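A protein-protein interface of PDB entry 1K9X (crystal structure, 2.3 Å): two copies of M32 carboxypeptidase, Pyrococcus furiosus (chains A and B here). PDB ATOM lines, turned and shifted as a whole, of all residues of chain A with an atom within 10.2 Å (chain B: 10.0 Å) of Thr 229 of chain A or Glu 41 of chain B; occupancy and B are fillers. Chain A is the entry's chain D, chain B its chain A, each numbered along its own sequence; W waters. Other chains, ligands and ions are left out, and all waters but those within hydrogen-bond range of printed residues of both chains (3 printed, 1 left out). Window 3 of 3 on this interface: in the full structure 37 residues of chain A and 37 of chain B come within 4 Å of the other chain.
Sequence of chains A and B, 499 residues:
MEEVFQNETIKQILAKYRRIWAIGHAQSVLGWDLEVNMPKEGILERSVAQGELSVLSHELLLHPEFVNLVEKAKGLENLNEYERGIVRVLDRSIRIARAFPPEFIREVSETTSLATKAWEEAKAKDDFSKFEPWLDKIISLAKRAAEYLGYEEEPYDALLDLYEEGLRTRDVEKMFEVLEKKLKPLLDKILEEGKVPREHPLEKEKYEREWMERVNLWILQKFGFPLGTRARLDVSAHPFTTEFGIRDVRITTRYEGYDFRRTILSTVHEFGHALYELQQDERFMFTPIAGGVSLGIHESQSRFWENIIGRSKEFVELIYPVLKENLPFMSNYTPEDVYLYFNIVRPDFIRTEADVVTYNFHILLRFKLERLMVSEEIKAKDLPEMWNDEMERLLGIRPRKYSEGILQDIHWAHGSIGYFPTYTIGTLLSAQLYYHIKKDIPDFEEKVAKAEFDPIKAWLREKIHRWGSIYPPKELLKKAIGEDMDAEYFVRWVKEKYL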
ATOM      1  N   TRP A  21       1.653 -28.457  -6.173  1.00  0.00           N
ATOM      2  CA  TRP A  21       2.136 -27.223  -6.770  1.00  0.00           C
ATOM      3  C   TRP A  21       3.636 -27.358  -7.041  1.00  0.00           C
ATOM      4  O   TRP A  21       4.122 -27.064  -8.138  1.00  0.00           O
ATOM      5  CB  TRP A  21       1.890 -26.040  -5.832  1.00  0.00           C
ATOM      6  CG  TRP A  21       2.477 -24.774  -6.358  1.00  0.00           C
ATOM      7  CD1 TRP A  21       1.900 -23.900  -7.243  1.00  0.00           C
ATOM      8  CD2 TRP A  21       3.800 -24.284  -6.114  1.00  0.00           C
ATOM      9  NE1 TRP A  21       2.785 -22.904  -7.565  1.00  0.00           N
ATOM     10  CE2 TRP A  21       3.960 -23.112  -6.888  1.00  0.00           C
ATOM     11  CE3 TRP A  21       4.867 -24.724  -5.316  1.00  0.00           C
ATOM     12  CZ2 TRP A  21       5.147 -22.370  -6.889  1.00  0.00           C
ATOM     13  CZ3 TRP A  21       6.052 -23.983  -5.315  1.00  0.00           C
ATOM     14  CH2 TRP A  21       6.181 -22.818  -6.101  1.00  0.00           C
ATOM     15  N   HIS A  25       5.985 -26.820 -10.431  1.00  0.00           N
ATOM     16  CA  HIS A  25       7.063 -25.843 -10.577  1.00  0.00           C
ATOM     17  C   HIS A  25       8.258 -26.543 -11.239  1.00  0.00           C
ATOM     18  O   HIS A  25       8.880 -26.014 -12.173  1.00  0.00           O
ATOM     19  CB  HIS A  25       7.426 -25.321  -9.188  1.00  0.00           C
ATOM     20  CG  HIS A  25       8.525 -24.308  -9.171  1.00  0.00           C
ATOM     21  ND1 HIS A  25       8.297 -22.959  -9.343  1.00  0.00           N
ATOM     22  CD2 HIS A  25       9.854 -24.440  -8.941  1.00  0.00           C
ATOM     23  CE1 HIS A  25       9.438 -22.304  -9.217  1.00  0.00           C
ATOM     24  NE2 HIS A  25      10.398 -23.181  -8.972  1.00  0.00           N
ATOM     25  N   GLY A 224       7.430  -2.293 -19.675  1.00  0.00           N
ATOM     26  CA  GLY A 224       7.681  -2.405 -18.247  1.00  0.00           C
ATOM     27  C   GLY A 224       7.840  -3.852 -17.801  1.00  0.00           C
ATOM     28  O   GLY A 224       7.514  -4.199 -16.674  1.00  0.00           O
ATOM     29  N   PHE A 225       8.334  -4.699 -18.697  1.00  0.00           N
ATOM     30  CA  PHE A 225       8.555  -6.115 -18.407  1.00  0.00           C
ATOM     31  C   PHE A 225       9.675  -6.229 -17.355  1.00  0.00           C
ATOM     32  O   PHE A 225      10.805  -5.802 -17.589  1.00  0.00           O
ATOM     33  CB  PHE A 225       8.947  -6.816 -19.705  1.00  0.00           C
ATOM     34  CG  PHE A 225       8.812  -8.309 -19.668  1.00  0.00           C
ATOM     35  CD1 PHE A 225       7.632  -8.907 -19.249  1.00  0.00           C
ATOM     36  CD2 PHE A 225       9.857  -9.115 -20.108  1.00  0.00           C
ATOM     37  CE1 PHE A 225       7.487 -10.291 -19.271  1.00  0.00           C
ATOM     38  CE2 PHE A 225       9.730 -10.496 -20.139  1.00  0.00           C
ATOM     39  CZ  PHE A 225       8.537 -11.092 -19.719  1.00  0.00           C
ATOM     40  N   PRO A 226       9.376  -6.821 -16.183  1.00  0.00           N
ATOM     41  CA  PRO A 226      10.354  -6.981 -15.087  1.00  0.00           C
ATOM     42  C   PRO A 226      11.545  -7.902 -15.381  1.00  0.00           C
ATOM     43  O   PRO A 226      11.786  -8.874 -14.662  1.00  0.00           O
ATOM     44  CB  PRO A 226       9.495  -7.502 -13.944  1.00  0.00           C
ATOM     45  CG  PRO A 226       8.535  -8.422 -14.686  1.00  0.00           C
ATOM     46  CD  PRO A 226       8.141  -7.580 -15.902  1.00  0.00           C
ATOM     47  N   LEU A 227      12.284  -7.574 -16.434  1.00  0.00           N
ATOM     48  CA  LEU A 227      13.457  -8.332 -16.862  1.00  0.00           C
ATOM     49  C   LEU A 227      14.504  -8.484 -15.744  1.00  0.00           C
ATOM     50  O   LEU A 227      14.887  -7.505 -15.116  1.00  0.00           O
ATOM     51  CB  LEU A 227      14.083  -7.623 -18.071  1.00  0.00           C
ATOM     52  CG  LEU A 227      14.130  -8.317 -19.437  1.00  0.00           C
ATOM     53  CD1 LEU A 227      13.032  -9.363 -19.574  1.00  0.00           C
ATOM     54  CD2 LEU A 227      14.006  -7.252 -20.538  1.00  0.00           C
ATOM     55  N   GLY A 228      14.959  -9.718 -15.516  1.00  0.00           N
ATOM     56  CA  GLY A 228      15.969  -9.992 -14.499  1.00  0.00           C
ATOM     57  C   GLY A 228      15.441  -9.978 -13.078  1.00  0.00           C
ATOM     58  O   GLY A 228      16.052 -10.509 -12.158  1.00  0.00           O
ATOM     59  N   THR A 229      14.281  -9.372 -12.907  1.00  0.00           N
ATOM     60  CA  THR A 229      13.653  -9.264 -11.600  1.00  0.00           C
ATOM     61  C   THR A 229      12.545 -10.300 -11.368  1.00  0.00           C
ATOM     62  O   THR A 229      12.543 -11.005 -10.356  1.00  0.00           O
ATOM     63  CB  THR A 229      13.112  -7.836 -11.425  1.00  0.00           C
ATOM     64  OG1 THR A 229      14.158  -7.000 -10.901  1.00  0.00           O
ATOM     65  CG2 THR A 229      11.926  -7.817 -10.513  1.00  0.00           C
ATOM     66  N   ARG A 230      11.598 -10.381 -12.297  1.00  0.00           N
ATOM     67  CA  ARG A 230      10.508 -11.338 -12.179  1.00  0.00           C
ATOM     68  C   ARG A 230      10.215 -12.037 -13.503  1.00  0.00           C
ATOM     69  O   ARG A 230       9.309 -12.866 -13.584  1.00  0.00           O
ATOM     70  CB  ARG A 230       9.248 -10.647 -11.654  1.00  0.00           C
ATOM     71  CG  ARG A 230       9.312 -10.337 -10.157  1.00  0.00           C
ATOM     72  CD  ARG A 230       8.074  -9.596  -9.694  1.00  0.00           C
ATOM     73  NE  ARG A 230       8.021  -8.256 -10.266  1.00  0.00           N
ATOM     74  CZ  ARG A 230       6.948  -7.728 -10.847  1.00  0.00           C
ATOM     75  NH1 ARG A 230       5.829  -8.429 -10.941  1.00  0.00           N
ATOM     76  NH2 ARG A 230       6.992  -6.495 -11.337  1.00  0.00           N
ATOM     77  N   ALA A 231      10.996 -11.717 -14.531  1.00  0.00           N
ATOM     78  CA  ALA A 231      10.804 -12.315 -15.847  1.00  0.00           C
ATOM     79  C   ALA A 231      12.095 -12.405 -16.648  1.00  0.00           C
ATOM     80  O   ALA A 231      13.085 -11.736 -16.333  1.00  0.00           O
ATOM     81  CB  ALA A 231       9.766 -11.527 -16.625  1.00  0.00           C
ATOM     82  N   ARG A 232      12.077 -13.245 -17.679  1.00  0.00           N
ATOM     83  CA  ARG A 232      13.231 -13.436 -18.558  1.00  0.00           C
ATOM     84  C   ARG A 232      12.785 -13.505 -20.009  1.00  0.00           C
ATOM     85  O   ARG A 232      11.620 -13.775 -20.299  1.00  0.00           O
ATOM     86  CB  ARG A 232      13.942 -14.765 -18.281  1.00  0.00           C
ATOM     87  CG  ARG A 232      14.796 -14.882 -17.051  1.00  0.00           C
ATOM     88  CD  ARG A 232      15.502 -16.245 -17.088  1.00  0.00           C
ATOM     89  NE  ARG A 232      16.364 -16.354 -18.264  1.00  0.00           N
ATOM     90  CZ  ARG A 232      17.627 -15.932 -18.306  1.00  0.00           C
ATOM     91  NH1 ARG A 232      18.184 -15.387 -17.229  1.00  0.00           N
ATOM     92  NH2 ARG A 232      18.323 -16.015 -19.433  1.00  0.00           N
ATOM     93  N   LEU A 233      13.722 -13.262 -20.917  1.00  0.00           N
ATOM     94  CA  LEU A 233      13.460 -13.385 -22.344  1.00  0.00           C
ATOM     95  C   LEU A 233      14.576 -14.300 -22.830  1.00  0.00           C
ATOM     96  O   LEU A 233      15.746 -14.061 -22.535  1.00  0.00           O
ATOM     97  CB  LEU A 233      13.552 -12.046 -23.089  1.00  0.00           C
ATOM     98  CG  LEU A 233      13.412 -12.197 -24.621  1.00  0.00           C
ATOM     99  CD1 LEU A 233      11.974 -12.537 -24.972  1.00  0.00           C
ATOM    100  CD2 LEU A 233      13.834 -10.916 -25.341  1.00  0.00           C
ATOM    101  N   PHE A 244       6.787 -20.063 -13.660  1.00  0.00           N
ATOM    102  CA  PHE A 244       7.428 -20.832 -12.607  1.00  0.00           C
ATOM    103  C   PHE A 244       6.776 -20.408 -11.307  1.00  0.00           C
ATOM    104  O   PHE A 244       6.723 -21.173 -10.346  1.00  0.00           O
ATOM    105  CB  PHE A 244       8.934 -20.545 -12.559  1.00  0.00           C
ATOM    106  CG  PHE A 244       9.696 -21.075 -13.739  1.00  0.00           C
ATOM    107  CD1 PHE A 244      11.082 -21.180 -13.692  1.00  0.00           C
ATOM    108  CD2 PHE A 244       9.035 -21.475 -14.905  1.00  0.00           C
ATOM    109  CE1 PHE A 244      11.803 -21.673 -14.783  1.00  0.00           C
ATOM    110  CE2 PHE A 244       9.752 -21.968 -16.001  1.00  0.00           C
ATOM    111  CZ  PHE A 244      11.141 -22.066 -15.935  1.00  0.00           C
ATOM    112  N   GLY A 245       6.277 -19.174 -11.302  1.00  0.00           N
ATOM    113  CA  GLY A 245       5.608 -18.614 -10.143  1.00  0.00           C
ATOM    114  C   GLY A 245       5.079 -17.227 -10.474  1.00  0.00           C
ATOM    115  O   GLY A 245       5.270 -16.723 -11.583  1.00  0.00           O
ATOM    116  N   ILE A 246       4.404 -16.598  -9.520  1.00  0.00           N
ATOM    117  CA  ILE A 246       3.886 -15.265  -9.763  1.00  0.00           C
ATOM    118  C   ILE A 246       5.057 -14.311  -9.979  1.00  0.00           C
ATOM    119  O   ILE A 246       4.952 -13.348 -10.738  1.00  0.00           O
ATOM    120  CB  ILE A 246       3.043 -14.776  -8.577  1.00  0.00           C
ATOM    121  CG1 ILE A 246       1.734 -15.568  -8.516  1.00  0.00           C
ATOM    122  CG2 ILE A 246       2.771 -13.277  -8.706  1.00  0.00           C
ATOM    123  CD1 ILE A 246       0.887 -15.243  -7.301  1.00  0.00           C
ATOM    124  N   ARG A 247       6.180 -14.619  -9.330  1.00  0.00           N
ATOM    125  CA  ARG A 247       7.390 -13.806  -9.405  1.00  0.00           C
ATOM    126  C   ARG A 247       8.475 -14.369 -10.325  1.00  0.00           C
ATOM    127  O   ARG A 247       9.645 -13.992 -10.211  1.00  0.00           O
ATOM    128  CB  ARG A 247       7.974 -13.631  -8.004  1.00  0.00           C
ATOM    129  CG  ARG A 247       7.113 -12.792  -7.067  1.00  0.00           C
ATOM    130  CD  ARG A 247       7.638 -12.863  -5.648  1.00  0.00           C
ATOM    131  NE  ARG A 247       6.831 -12.090  -4.708  1.00  0.00           N
ATOM    132  CZ  ARG A 247       7.012 -12.114  -3.392  1.00  0.00           C
ATOM    133  NH1 ARG A 247       7.965 -12.877  -2.870  1.00  0.00           N
ATOM    134  NH2 ARG A 247       6.249 -11.377  -2.595  1.00  0.00           N
ATOM    135  N   ASP A 248       8.096 -15.260 -11.236  1.00  0.00           N
ATOM    136  CA  ASP A 248       9.062 -15.852 -12.159  1.00  0.00           C
ATOM    137  C   ASP A 248       8.380 -16.358 -13.432  1.00  0.00           C
ATOM    138  O   ASP A 248       8.099 -17.548 -13.567  1.00  0.00           O
ATOM    139  CB  ASP A 248       9.784 -17.000 -11.464  1.00  0.00           C
ATOM    140  CG  ASP A 248      10.912 -17.569 -12.292  1.00  0.00           C
ATOM    141  OD1 ASP A 248      11.026 -17.222 -13.486  1.00  0.00           O
ATOM    142  OD2 ASP A 248      11.685 -18.379 -11.740  1.00  0.00           O
ATOM    143  N   VAL A 249       8.113 -15.441 -14.356  1.00  0.00           N
ATOM    144  CA  VAL A 249       7.457 -15.776 -15.608  1.00  0.00           C
ATOM    145  C   VAL A 249       8.418 -15.531 -16.755  1.00  0.00           C
ATOM    146  O   VAL A 249       9.003 -14.459 -16.863  1.00  0.00           O
ATOM    147  CB  VAL A 249       6.188 -14.920 -15.819  1.00  0.00           C
ATOM    148  CG1 VAL A 249       5.446 -15.398 -17.064  1.00  0.00           C
ATOM    149  CG2 VAL A 249       5.281 -15.023 -14.587  1.00  0.00           C
ATOM    150  N   ARG A 250       8.567 -16.531 -17.618  1.00  0.00           N
ATOM    151  CA  ARG A 250       9.488 -16.441 -18.733  1.00  0.00           C
ATOM    152  C   ARG A 250       8.824 -16.624 -20.092  1.00  0.00           C
ATOM    153  O   ARG A 250       7.829 -17.341 -20.230  1.00  0.00           O
ATOM    154  CB  ARG A 250      10.586 -17.488 -18.539  1.00  0.00           C
ATOM    155  CG  ARG A 250      11.079 -17.542 -17.098  1.00  0.00           C
ATOM    156  CD  ARG A 250      12.249 -18.488 -16.897  1.00  0.00           C
ATOM    157  NE  ARG A 250      12.643 -18.508 -15.490  1.00  0.00           N
ATOM    158  CZ  ARG A 250      13.664 -19.206 -14.990  1.00  0.00           C
ATOM    159  NH1 ARG A 250      14.420 -19.959 -15.775  1.00  0.00           N
ATOM    160  NH2 ARG A 250      13.920 -19.153 -13.693  1.00  0.00           N
ATOM    161  N   LEU A 278       2.011 -12.544 -14.416  1.00  0.00           N
ATOM    162  CA  LEU A 278       2.752 -11.624 -13.562  1.00  0.00           C
ATOM    163  C   LEU A 278       1.811 -10.885 -12.617  1.00  0.00           C
ATOM    164  O   LEU A 278       2.167 -10.608 -11.463  1.00  0.00           O
ATOM    165  CB  LEU A 278       3.500 -10.595 -14.413  1.00  0.00           C
ATOM    166  CG  LEU A 278       5.028 -10.550 -14.588  1.00  0.00           C
ATOM    167  CD1 LEU A 278       5.703 -11.824 -14.124  1.00  0.00           C
ATOM    168  CD2 LEU A 278       5.334 -10.281 -16.067  1.00  0.00           C
ATOM    169  N   GLU A 282      -0.855 -12.036  -5.379  1.00  0.00           N
ATOM    170  CA  GLU A 282       0.134 -12.777  -4.597  1.00  0.00           C
ATOM    171  C   GLU A 282      -0.397 -13.485  -3.342  1.00  0.00           C
ATOM    172  O   GLU A 282       0.278 -14.360  -2.790  1.00  0.00           O
ATOM    173  CB  GLU A 282       1.333 -11.872  -4.236  1.00  0.00           C
ATOM    174  CG  GLU A 282       2.134 -11.417  -5.468  1.00  0.00           C
ATOM    175  CD  GLU A 282       3.488 -10.790  -5.135  1.00  0.00           C
ATOM    176  OE1 GLU A 282       3.591 -10.054  -4.135  1.00  0.00           O
ATOM    177  OE2 GLU A 282       4.457 -11.018  -5.890  1.00  0.00           O
ATOM    178  N   MET A 285      -0.577 -17.166  -3.868  1.00  0.00           N
ATOM    179  CA  MET A 285       0.652 -17.907  -4.122  1.00  0.00           C
ATOM    180  C   MET A 285       0.601 -19.361  -3.625  1.00  0.00           C
ATOM    181  O   MET A 285       0.133 -19.640  -2.521  1.00  0.00           O
ATOM    182  CB  MET A 285       1.820 -17.174  -3.462  1.00  0.00           C
ATOM    183  CG  MET A 285       3.181 -17.612  -3.940  1.00  0.00           C
ATOM    184  SD  MET A 285       4.487 -16.554  -3.308  1.00  0.00           S
ATOM    185  CE  MET A 285       4.625 -15.332  -4.632  1.00  0.00           C
ATOM    186  N   PHE A 286       1.080 -20.285  -4.450  1.00  0.00           N
ATOM    187  CA  PHE A 286       1.109 -21.706  -4.100  1.00  0.00           C
ATOM    188  C   PHE A 286      -0.252 -22.392  -4.119  1.00  0.00           C
ATOM    189  O   PHE A 286      -0.335 -23.576  -3.823  1.00  0.00           O
ATOM    190  CB  PHE A 286       1.718 -21.908  -2.699  1.00  0.00           C
ATOM    191  CG  PHE A 286       3.046 -21.241  -2.503  1.00  0.00           C
ATOM    192  CD1 PHE A 286       3.237 -20.361  -1.439  1.00  0.00           C
ATOM    193  CD2 PHE A 286       4.097 -21.471  -3.384  1.00  0.00           C
ATOM    194  CE1 PHE A 286       4.447 -19.719  -1.257  1.00  0.00           C
ATOM    195  CE2 PHE A 286       5.314 -20.832  -3.210  1.00  0.00           C
ATOM    196  CZ  PHE A 286       5.491 -19.951  -2.142  1.00  0.00           C
ATOM    197  N   ASP B  33      19.303 -23.879 -12.248  1.00  0.00           N
ATOM    198  CA  ASP B  33      18.590 -22.705 -12.749  1.00  0.00           C
ATOM    199  C   ASP B  33      18.630 -21.545 -11.769  1.00  0.00           C
ATOM    200  O   ASP B  33      18.797 -20.395 -12.167  1.00  0.00           O
ATOM    201  CB  ASP B  33      17.129 -23.051 -13.047  1.00  0.00           C
ATOM    202  CG  ASP B  33      16.324 -21.834 -13.474  1.00  0.00           C
ATOM    203  OD1 ASP B  33      15.714 -21.173 -12.605  1.00  0.00           O
ATOM    204  OD2 ASP B  33      16.324 -21.524 -14.683  1.00  0.00           O
ATOM    205  N   LEU B  34      18.461 -21.855 -10.489  1.00  0.00           N
ATOM    206  CA  LEU B  34      18.485 -20.837  -9.454  1.00  0.00           C
ATOM    207  C   LEU B  34      19.779 -20.020  -9.524  1.00  0.00           C
ATOM    208  O   LEU B  34      19.739 -18.795  -9.454  1.00  0.00           O
ATOM    209  CB  LEU B  34      18.302 -21.498  -8.080  1.00  0.00           C
ATOM    210  CG  LEU B  34      18.717 -20.830  -6.759  1.00  0.00           C
ATOM    211  CD1 LEU B  34      18.596 -19.325  -6.815  1.00  0.00           C
ATOM    212  CD2 LEU B  34      17.853 -21.398  -5.643  1.00  0.00           C
ATOM    213  N   ASN B  37      20.003 -18.799 -14.234  1.00  0.00           N
ATOM    214  CA  ASN B  37      19.049 -17.969 -14.966  1.00  0.00           C
ATOM    215  C   ASN B  37      17.934 -17.274 -14.195  1.00  0.00           C
ATOM    216  O   ASN B  37      17.452 -16.227 -14.622  1.00  0.00           O
ATOM    217  CB  ASN B  37      18.374 -18.811 -16.063  1.00  0.00           C
ATOM    218  CG  ASN B  37      19.348 -19.686 -16.825  1.00  0.00           C
ATOM    219  OD1 ASN B  37      20.204 -19.190 -17.556  1.00  0.00           O
ATOM    220  ND2 ASN B  37      19.214 -21.001 -16.664  1.00  0.00           N
ATOM    221  N   MET B  38      17.515 -17.863 -13.083  1.00  0.00           N
ATOM    222  CA  MET B  38      16.400 -17.342 -12.307  1.00  0.00           C
ATOM    223  C   MET B  38      16.358 -15.871 -11.917  1.00  0.00           C
ATOM    224  O   MET B  38      17.277 -15.366 -11.280  1.00  0.00           O
ATOM    225  CB  MET B  38      16.221 -18.176 -11.034  1.00  0.00           C
ATOM    226  CG  MET B  38      14.970 -17.845 -10.271  1.00  0.00           C
ATOM    227  SD  MET B  38      14.917 -18.665  -8.667  1.00  0.00           S
ATOM    228  CE  MET B  38      15.959 -17.524  -7.718  1.00  0.00           C
ATOM    229  N   PRO B  39      15.280 -15.163 -12.306  1.00  0.00           N
ATOM    230  CA  PRO B  39      15.163 -13.743 -11.945  1.00  0.00           C
ATOM    231  C   PRO B  39      15.154 -13.709 -10.426  1.00  0.00           C
ATOM    232  O   PRO B  39      14.448 -14.496  -9.793  1.00  0.00           O
ATOM    233  CB  PRO B  39      13.824 -13.317 -12.562  1.00  0.00           C
ATOM    234  CG  PRO B  39      13.131 -14.638 -12.948  1.00  0.00           C
ATOM    235  CD  PRO B  39      14.261 -15.552 -13.296  1.00  0.00           C
ATOM    236  N   LYS B  40      15.940 -12.813  -9.844  1.00  0.00           N
ATOM    237  CA  LYS B  40      16.064 -12.754  -8.392  1.00  0.00           C
ATOM    238  C   LYS B  40      14.800 -12.909  -7.548  1.00  0.00           C
ATOM    239  O   LYS B  40      14.832 -13.579  -6.520  1.00  0.00           O
ATOM    240  CB  LYS B  40      16.859 -11.498  -7.971  1.00  0.00           C
ATOM    241  CG  LYS B  40      16.540 -10.237  -8.759  1.00  0.00           C
ATOM    242  CD  LYS B  40      15.637  -9.283  -7.981  1.00  0.00           C
ATOM    243  CE  LYS B  40      16.397  -8.558  -6.865  1.00  0.00           C
ATOM    244  NZ  LYS B  40      15.475  -7.704  -6.057  1.00  0.00           N
ATOM    245  N   GLU B  41      13.686 -12.327  -7.962  1.00  0.00           N
ATOM    246  CA  GLU B  41      12.481 -12.460  -7.155  1.00  0.00           C
ATOM    247  C   GLU B  41      11.814 -13.833  -7.231  1.00  0.00           C
ATOM    248  O   GLU B  41      10.803 -14.078  -6.565  1.00  0.00           O
ATOM    249  CB  GLU B  41      11.478 -11.362  -7.511  1.00  0.00           C
ATOM    250  CG  GLU B  41      11.875  -9.997  -6.972  1.00  0.00           C
ATOM    251  CD  GLU B  41      10.861  -8.914  -7.303  1.00  0.00           C
ATOM    252  OE1 GLU B  41       9.655  -9.132  -7.055  1.00  0.00           O
ATOM    253  OE2 GLU B  41      11.274  -7.841  -7.798  1.00  0.00           O
ATOM    254  N   GLY B  42      12.377 -14.736  -8.029  1.00  0.00           N
ATOM    255  CA  GLY B  42      11.805 -16.063  -8.124  1.00  0.00           C
ATOM    256  C   GLY B  42      12.212 -16.906  -6.930  1.00  0.00           C
ATOM    257  O   GLY B  42      11.681 -17.994  -6.721  1.00  0.00           O
ATOM    258  N   ILE B  43      13.128 -16.373  -6.121  1.00  0.00           N
ATOM    259  CA  ILE B  43      13.659 -17.082  -4.961  1.00  0.00           C
ATOM    260  C   ILE B  43      12.655 -17.619  -3.950  1.00  0.00           C
ATOM    261  O   ILE B  43      12.802 -18.750  -3.475  1.00  0.00           O
ATOM    262  CB  ILE B  43      14.726 -16.225  -4.206  1.00  0.00           C
ATOM    263  CG1 ILE B  43      15.415 -17.087  -3.144  1.00  0.00           C
ATOM    264  CG2 ILE B  43      14.071 -14.990  -3.546  1.00  0.00           C
ATOM    265  CD1 ILE B  43      16.093 -18.340  -3.713  1.00  0.00           C
ATOM    266  N   LEU B  44      11.637 -16.835  -3.613  1.00  0.00           N
ATOM    267  CA  LEU B  44      10.647 -17.289  -2.636  1.00  0.00           C
ATOM    268  C   LEU B  44       9.913 -18.552  -3.089  1.00  0.00           C
ATOM    269  O   LEU B  44       9.802 -19.520  -2.344  1.00  0.00           O
ATOM    270  CB  LEU B  44       9.629 -16.182  -2.344  1.00  0.00           C
ATOM    271  CG  LEU B  44       8.435 -16.631  -1.491  1.00  0.00           C
ATOM    272  CD1 LEU B  44       8.938 -17.287  -0.202  1.00  0.00           C
ATOM    273  CD2 LEU B  44       7.539 -15.444  -1.174  1.00  0.00           C
ATOM    274  N   GLU B  45       9.422 -18.550  -4.318  1.00  0.00           N
ATOM    275  CA  GLU B  45       8.698 -19.706  -4.818  1.00  0.00           C
ATOM    276  C   GLU B  45       9.604 -20.898  -5.123  1.00  0.00           C
ATOM    277  O   GLU B  45       9.225 -22.044  -4.886  1.00  0.00           O
ATOM    278  CB  GLU B  45       7.849 -19.295  -6.024  1.00  0.00           C
ATOM    279  CG  GLU B  45       6.594 -18.513  -5.580  1.00  0.00           C
ATOM    280  CD  GLU B  45       6.037 -17.611  -6.658  1.00  0.00           C
ATOM    281  OE1 GLU B  45       6.819 -16.786  -7.185  1.00  0.00           O
ATOM    282  OE2 GLU B  45       4.824 -17.720  -6.976  1.00  0.00           O
ATOM    283  N   ARG B  46      10.803 -20.643  -5.631  1.00  0.00           N
ATOM    284  CA  ARG B  46      11.709 -21.748  -5.897  1.00  0.00           C
ATOM    285  C   ARG B  46      11.991 -22.454  -4.558  1.00  0.00           C
ATOM    286  O   ARG B  46      11.988 -23.683  -4.481  1.00  0.00           O
ATOM    287  CB  ARG B  46      13.011 -21.236  -6.522  1.00  0.00           C
ATOM    288  CG  ARG B  46      14.075 -22.302  -6.711  1.00  0.00           C
ATOM    289  CD  ARG B  46      13.651 -23.371  -7.706  1.00  0.00           C
ATOM    290  NE  ARG B  46      14.141 -23.099  -9.055  1.00  0.00           N
ATOM    291  CZ  ARG B  46      13.499 -22.377  -9.965  1.00  0.00           C
ATOM    292  NH1 ARG B  46      12.322 -21.844  -9.696  1.00  0.00           N
ATOM    293  NH2 ARG B  46      14.045 -22.174 -11.147  1.00  0.00           N
ATOM    294  N   SER B  47      12.190 -21.662  -3.506  1.00  0.00           N
ATOM    295  CA  SER B  47      12.483 -22.175  -2.167  1.00  0.00           C
ATOM    296  C   SER B  47      11.474 -23.166  -1.619  1.00  0.00           C
ATOM    297  O   SER B  47      11.853 -24.247  -1.153  1.00  0.00           O
ATOM    298  CB  SER B  47      12.608 -21.027  -1.154  1.00  0.00           C
ATOM    299  OG  SER B  47      13.778 -20.263  -1.376  1.00  0.00           O
HETATM  300  O   HOH W   1      11.146 -19.585  -9.586  1.00  0.00           O
HETATM  301  O   HOH W   2      10.645 -13.542  -3.963  1.00  0.00           O
HETATM  302  O   HOH W   3       2.903 -19.656  -6.960  1.00  0.00           O
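N of Lys 40 of chain B lies within hydrogen-bond range of O of Gly 228 of chain A, at 3.3 Å. A ring nitrogen (NE2) of His 25 of chain A is in hydrogen-bond range of the guanidinium group of Arg 46 of chain B (2.5 Å). The backbone carbonyl oxygen (O) of Asn 37 of chain B is in hydrogen-bond range of the guanidinium group (NH1) of Arg 232 of chain A, 2.8 Å away. N of Glu 41 of chain B lies within hydrogen-bond range of O of Thr 229 of chain A (3.0 Å). The side-chain carboxylate of Glu 45 of chain B lies within hydrogen-bond range of the backbone NH of Arg 247 of chain A (3.1 Å). The side-chain carboxylate of Glu 45 of chain B is in hydrogen-bond range of the backbone NH of Ile 246 of chain A.
Water W1 lies within hydrogen-bond range of OD2 of Asp 248 of chain A, NH1 of Arg 46 of chain B and O of Gly 42 of chain B.
Hydrophobic or aromatic side chains of chain A that line the printed part of chain B: Trp 21, His 25, Ile 246, Met 285 and Phe 286. Along chain A the printed residues that touch a printed residue of chain B span positions 21 to 286. Printed residues of chain B that touch a printed residue of chain A: Asp 33, Asn 37, Met 38, Pro 39, Lys 40, Glu 41, Gly 42, Leu 44, Glu 45 and Arg 46. Hydrophobic or aromatic side chains of chain B within 4 Å of the printed part of chain A: Met 38, Pro 39 and Leu 44. Among the printed residues, 27 pairs touch across the chains. Among the printed residues, Asp or Glu carboxylates within 4 Å of a Lys or Arg side-chain nitrogen of the other chain: Arg 230 of chain A with Glu 41 of chain B and Arg 250 of chain A with Asp 33 of chain B.
Thr 229 of chain A touches three residues of chain B. Of chain A, only Gly 228 (3.3 Å) and Thr 229 (3.9 Å) come within 4 Å of Lys 40 of chain B. Printed residues of chain B within 4 Å of Ile 246 of chain A: Glu 45 (2.8 Å). Printed residues of chain B within 4 Å of Gly 245 of chain A: Glu 45 (3.4 Å). Of the printed residues of chain B, Asp 248 of chain A touches Met 38 and Pro 39. The nearest residue of chain A that does not touch Glu 41 of chain B is Gly 228 of chain A (5.1 Å).
No position is printed for both chains. Of the 27 pairs that touch across the chains among the printed residues, none has its exchanged pair printed and touching as well.
Gly 245 of chain A touches Glu 45 of chain B (CA to OE2, 3.4 Å). Arg 247 of chain A touches Glu 41 of chain B (CB to O, 3.2 Å). CD2 of Leu 44 of chain B touches NH1 of Arg 247 of chain A, 3.1 Å away.
The backbone carbonyl oxygen (O) of Phe 244 of chain A sits at hydrogen-bond distance from a ring nitrogen (ND1) of His 25 of chain A (2.6 Å).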
